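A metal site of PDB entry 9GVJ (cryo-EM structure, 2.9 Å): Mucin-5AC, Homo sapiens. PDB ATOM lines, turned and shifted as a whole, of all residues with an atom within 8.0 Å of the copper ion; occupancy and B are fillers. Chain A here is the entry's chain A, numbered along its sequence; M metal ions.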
ATOM      1  N   PRO A  47       9.029 -38.566  17.710  1.00  0.00           N
ATOM      2  CA  PRO A  47       8.905 -37.164  18.116  1.00  0.00           C
ATOM      3  C   PRO A  47       9.943 -36.714  19.122  1.00  0.00           C
ATOM      4  O   PRO A  47      10.035 -35.512  19.398  1.00  0.00           O
ATOM      5  CB  PRO A  47       7.492 -37.097  18.705  1.00  0.00           C
ATOM      6  CG  PRO A  47       7.212 -38.526  19.190  1.00  0.00           C
ATOM      7  CD  PRO A  47       8.284 -39.446  18.634  1.00  0.00           C
ATOM      8  N   ALA A  48      10.741 -37.631  19.674  1.00  0.00           N
ATOM      9  CA  ALA A  48      11.823 -37.251  20.574  1.00  0.00           C
ATOM     10  C   ALA A  48      12.973 -36.663  19.769  1.00  0.00           C
ATOM     11  O   ALA A  48      13.653 -37.382  19.038  1.00  0.00           O
ATOM     12  CB  ALA A  48      12.289 -38.461  21.374  1.00  0.00           C
ATOM     13  N   HIS A  49      13.178 -35.351  19.901  1.00  0.00           N
ATOM     14  CA  HIS A  49      14.188 -34.640  19.138  1.00  0.00           C
ATOM     15  C   HIS A  49      15.149 -33.909  20.061  1.00  0.00           C
ATOM     16  O   HIS A  49      15.526 -32.765  19.811  1.00  0.00           O
ATOM     17  CB  HIS A  49      13.538 -33.670  18.143  1.00  0.00           C
ATOM     18  CG  HIS A  49      12.602 -32.688  18.790  1.00  0.00           C
ATOM     19  ND1 HIS A  49      11.253 -32.945  18.949  1.00  0.00           N
ATOM     20  CD2 HIS A  49      12.821 -31.470  19.308  1.00  0.00           C
ATOM     21  CE1 HIS A  49      10.687 -31.916  19.541  1.00  0.00           C
ATOM     22  NE2 HIS A  49      11.609 -30.996  19.768  1.00  0.00           N
ATOM     23  N   ASN A  50      15.556 -34.571  21.139  1.00  0.00           N
ATOM     24  CA  ASN A  50      16.525 -33.976  22.052  1.00  0.00           C
ATOM     25  C   ASN A  50      17.896 -33.803  21.410  1.00  0.00           C
ATOM     26  O   ASN A  50      18.703 -33.015  21.915  1.00  0.00           O
ATOM     27  CB  ASN A  50      16.656 -34.821  23.322  1.00  0.00           C
ATOM     28  CG  ASN A  50      15.868 -34.253  24.480  1.00  0.00           C
ATOM     29  OD1 ASN A  50      16.078 -33.108  24.890  1.00  0.00           O
ATOM     30  ND2 ASN A  50      14.970 -35.041  25.033  1.00  0.00           N
ATOM     31  N   ARG A  52      18.482 -32.380  18.618  1.00  0.00           N
ATOM     32  CA  ARG A  52      18.498 -31.129  17.889  1.00  0.00           C
ATOM     33  C   ARG A  52      18.535 -29.908  18.804  1.00  0.00           C
ATOM     34  O   ARG A  52      18.479 -28.783  18.313  1.00  0.00           O
ATOM     35  CB  ARG A  52      17.273 -31.040  16.973  1.00  0.00           C
ATOM     36  CG  ARG A  52      17.269 -32.025  15.833  1.00  0.00           C
ATOM     37  CD  ARG A  52      15.897 -32.062  15.178  1.00  0.00           C
ATOM     38  NE  ARG A  52      15.332 -30.721  15.053  1.00  0.00           N
ATOM     39  CZ  ARG A  52      14.073 -30.412  15.324  1.00  0.00           C
ATOM     40  NH1 ARG A  52      13.206 -31.324  15.735  1.00  0.00           N
ATOM     41  NH2 ARG A  52      13.664 -29.158  15.187  1.00  0.00           N
ATOM     42  N   VAL A  53      18.625 -30.125  20.114  1.00  0.00           N
ATOM     43  CA  VAL A  53      18.508 -29.045  21.093  1.00  0.00           C
ATOM     44  C   VAL A  53      19.778 -28.975  21.909  1.00  0.00           C
ATOM     45  O   VAL A  53      20.233 -29.986  22.463  1.00  0.00           O
ATOM     46  CB  VAL A  53      17.279 -29.254  22.013  1.00  0.00           C
ATOM     47  CG1 VAL A  53      17.240 -28.185  23.092  1.00  0.00           C
ATOM     48  CG2 VAL A  53      16.002 -29.244  21.191  1.00  0.00           C
ATOM     49  N   VAL A 159      15.958 -21.750  16.116  1.00  0.00           N
ATOM     50  CA  VAL A 159      15.165 -21.079  17.133  1.00  0.00           C
ATOM     51  C   VAL A 159      16.037 -20.888  18.364  1.00  0.00           C
ATOM     52  O   VAL A 159      16.599 -21.860  18.888  1.00  0.00           O
ATOM     53  CB  VAL A 159      13.892 -21.856  17.500  1.00  0.00           C
ATOM     54  CG1 VAL A 159      13.111 -21.121  18.571  1.00  0.00           C
ATOM     55  CG2 VAL A 159      13.023 -22.064  16.263  1.00  0.00           C
ATOM     56  N   LEU A 169      18.577 -21.568  25.103  1.00  0.00           N
ATOM     57  CA  LEU A 169      18.277 -22.837  24.446  1.00  0.00           C
ATOM     58  C   LEU A 169      18.240 -22.627  22.944  1.00  0.00           C
ATOM     59  O   LEU A 169      17.560 -21.728  22.456  1.00  0.00           O
ATOM     60  CB  LEU A 169      16.949 -23.407  24.950  1.00  0.00           C
ATOM     61  CG  LEU A 169      16.608 -24.834  24.535  1.00  0.00           C
ATOM     62  CD1 LEU A 169      16.121 -25.637  25.734  1.00  0.00           C
ATOM     63  CD2 LEU A 169      15.559 -24.837  23.434  1.00  0.00           C
ATOM     64  N   GLU A 171      17.568 -24.561  19.217  1.00  0.00           N
ATOM     65  CA  GLU A 171      17.029 -25.686  18.478  1.00  0.00           C
ATOM     66  C   GLU A 171      17.354 -25.493  17.007  1.00  0.00           C
ATOM     67  O   GLU A 171      17.030 -24.452  16.425  1.00  0.00           O
ATOM     68  CB  GLU A 171      15.524 -25.822  18.695  1.00  0.00           C
ATOM     69  CG  GLU A 171      14.927 -27.085  18.101  1.00  0.00           C
ATOM     70  CD  GLU A 171      13.443 -26.958  17.836  1.00  0.00           C
ATOM     71  OE1 GLU A 171      12.676 -26.722  18.788  1.00  0.00           O
ATOM     72  OE2 GLU A 171      13.039 -27.076  16.657  1.00  0.00           O
ATOM     73  N   ARG A 289      11.895 -28.759  30.353  1.00  0.00           N
ATOM     74  CA  ARG A 289      12.059 -28.342  28.962  1.00  0.00           C
ATOM     75  C   ARG A 289      12.541 -29.498  28.092  1.00  0.00           C
ATOM     76  O   ARG A 289      12.033 -29.710  26.986  1.00  0.00           O
ATOM     77  CB  ARG A 289      13.040 -27.171  28.891  1.00  0.00           C
ATOM     78  CG  ARG A 289      12.623 -26.047  27.959  1.00  0.00           C
ATOM     79  CD  ARG A 289      13.078 -24.701  28.502  1.00  0.00           C
ATOM     80  NE  ARG A 289      14.313 -24.818  29.270  1.00  0.00           N
ATOM     81  CZ  ARG A 289      14.601 -24.069  30.335  1.00  0.00           C
ATOM     82  NH1 ARG A 289      13.765 -23.155  30.776  1.00  0.00           N
ATOM     83  NH2 ARG A 289      15.761 -24.256  30.950  1.00  0.00           N
ATOM     84  N   GLN A 290      13.527 -30.252  28.588  1.00  0.00           N
ATOM     85  CA  GLN A 290      14.039 -31.383  27.818  1.00  0.00           C
ATOM     86  C   GLN A 290      12.975 -32.459  27.666  1.00  0.00           C
ATOM     87  O   GLN A 290      12.893 -33.120  26.625  1.00  0.00           O
ATOM     88  CB  GLN A 290      15.288 -31.946  28.496  1.00  0.00           C
ATOM     89  CG  GLN A 290      16.408 -30.937  28.697  1.00  0.00           C
ATOM     90  CD  GLN A 290      16.861 -30.298  27.397  1.00  0.00           C
ATOM     91  OE1 GLN A 290      16.934 -30.947  26.358  1.00  0.00           O
ATOM     92  NE2 GLN A 290      17.166 -29.003  27.455  1.00  0.00           N
ATOM     93  N   THR A 292       9.743 -31.874  27.477  1.00  0.00           N
ATOM     94  CA  THR A 292       8.866 -31.368  26.420  1.00  0.00           C
ATOM     95  C   THR A 292       9.490 -31.601  25.048  1.00  0.00           C
ATOM     96  O   THR A 292       8.793 -31.963  24.098  1.00  0.00           O
ATOM     97  CB  THR A 292       8.578 -29.879  26.624  1.00  0.00           C
ATOM     98  OG1 THR A 292       9.802 -29.141  26.606  1.00  0.00           O
ATOM     99  CG2 THR A 292       7.853 -29.648  27.947  1.00  0.00           C
ATOM    100  N   HIS A 293      10.800 -31.396  24.923  1.00  0.00           N
ATOM    101  CA  HIS A 293      11.474 -31.641  23.661  1.00  0.00           C
ATOM    102  C   HIS A 293      11.592 -33.123  23.337  1.00  0.00           C
ATOM    103  O   HIS A 293      11.918 -33.480  22.198  1.00  0.00           O
ATOM    104  CB  HIS A 293      12.857 -30.998  23.659  1.00  0.00           C
ATOM    105  CG  HIS A 293      12.839 -29.524  23.432  1.00  0.00           C
ATOM    106  ND1 HIS A 293      12.336 -28.953  22.280  1.00  0.00           N
ATOM    107  CD2 HIS A 293      13.246 -28.486  24.204  1.00  0.00           C
ATOM    108  CE1 HIS A 293      12.438 -27.639  22.350  1.00  0.00           C
ATOM    109  NE2 HIS A 293      12.998 -27.331  23.506  1.00  0.00           N
ATOM    110  N   ALA A 294      11.326 -33.999  24.307  1.00  0.00           N
ATOM    111  CA  ALA A 294      11.414 -35.443  24.107  1.00  0.00           C
ATOM    112  C   ALA A 294      10.077 -36.067  23.719  1.00  0.00           C
ATOM    113  O   ALA A 294      10.000 -37.293  23.575  1.00  0.00           O
ATOM    114  CB  ALA A 294      11.931 -36.122  25.383  1.00  0.00           C
ATOM    115  N   GLY A 295       9.036 -35.267  23.529  1.00  0.00           N
ATOM    116  CA  GLY A 295       7.717 -35.797  23.246  1.00  0.00           C
ATOM    117  C   GLY A 295       6.903 -36.167  24.469  1.00  0.00           C
ATOM    118  O   GLY A 295       5.870 -36.840  24.315  1.00  0.00           O
ATOM    119  N   ASP A 339       3.679 -27.484  16.467  1.00  0.00           N
ATOM    120  CA  ASP A 339       4.729 -27.593  17.455  1.00  0.00           C
ATOM    121  C   ASP A 339       4.251 -28.419  18.654  1.00  0.00           C
ATOM    122  O   ASP A 339       3.048 -28.620  18.865  1.00  0.00           O
ATOM    123  CB  ASP A 339       5.178 -26.214  17.928  1.00  0.00           C
ATOM    124  CG  ASP A 339       5.877 -25.429  16.826  1.00  0.00           C
ATOM    125  OD1 ASP A 339       6.317 -26.045  15.840  1.00  0.00           O
ATOM    126  OD2 ASP A 339       5.989 -24.195  16.962  1.00  0.00           O
ATOM    127  N   HIS A 340       5.210 -28.891  19.439  1.00  0.00           N
ATOM    128  CA  HIS A 340       4.895 -29.628  20.654  1.00  0.00           C
ATOM    129  C   HIS A 340       4.596 -28.666  21.804  1.00  0.00           C
ATOM    130  O   HIS A 340       4.799 -27.456  21.701  1.00  0.00           O
ATOM    131  CB  HIS A 340       6.048 -30.561  21.023  1.00  0.00           C
ATOM    132  CG  HIS A 340       7.354 -29.862  21.244  1.00  0.00           C
ATOM    133  ND1 HIS A 340       7.648 -29.181  22.415  1.00  0.00           N
ATOM    134  CD2 HIS A 340       8.438 -29.728  20.451  1.00  0.00           C
ATOM    135  CE1 HIS A 340       8.858 -28.661  22.323  1.00  0.00           C
ATOM    136  NE2 HIS A 340       9.367 -28.983  21.145  1.00  0.00           N
ATOM    137  N   CYS A 341       4.101 -29.226  22.895  1.00  0.00           N
ATOM    138  CA  CYS A 341       3.727 -28.417  24.047  1.00  0.00           C
ATOM    139  C   CYS A 341       4.956 -27.767  24.676  1.00  0.00           C
ATOM    140  O   CYS A 341       6.065 -28.308  24.628  1.00  0.00           O
ATOM    141  CB  CYS A 341       2.990 -29.268  25.082  1.00  0.00           C
ATOM    142  SG  CYS A 341       4.051 -30.050  26.309  1.00  0.00           S
ATOM    143  N   VAL A 342       4.744 -26.597  25.277  1.00  0.00           N
ATOM    144  CA  VAL A 342       5.804 -25.834  25.926  1.00  0.00           C
ATOM    145  C   VAL A 342       5.289 -25.333  27.272  1.00  0.00           C
ATOM    146  O   VAL A 342       4.129 -25.500  27.621  1.00  0.00           O
ATOM    147  CB  VAL A 342       6.286 -24.650  25.063  1.00  0.00           C
ATOM    148  CG1 VAL A 342       7.084 -25.149  23.864  1.00  0.00           C
ATOM    149  CG2 VAL A 342       5.111 -23.799  24.628  1.00  0.00           C
HETATM  150 CU    CU M   1      11.373 -28.892  20.295  1.00  0.00          CU
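O of Thr 292 sits at hydrogen-bond distance from ND1 of His 340, 3.4 Å away. A ring nitrogen (ND1) of His 49 is in hydrogen-bond range of the backbone carbonyl oxygen of Pro 47, 2.9 Å away. The side-chain carboxylate (OE2) of Glu 171 is in salt-bridge range of the guanidinium group (NH2) of Arg 52 (2.6 Å). The backbone NH (N) of Glu 171 sits at hydrogen-bond distance from the backbone carbonyl oxygen (O) of Val 159 (2.9 Å).
OE1 of Glu 171 touches the copper ion (2.9 Å). Within 4 Å of the copper ion: His 49, Glu 171, His 293 and His 340. The nearest printed residue that does not touch the copper ion is Val 53 (4.7 Å).
The copper ion is bound by NE2 of His 340 (2.2 Å), NE2 of His 49 (2.2 Å) and ND1 of His 293 (2.2 Å).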
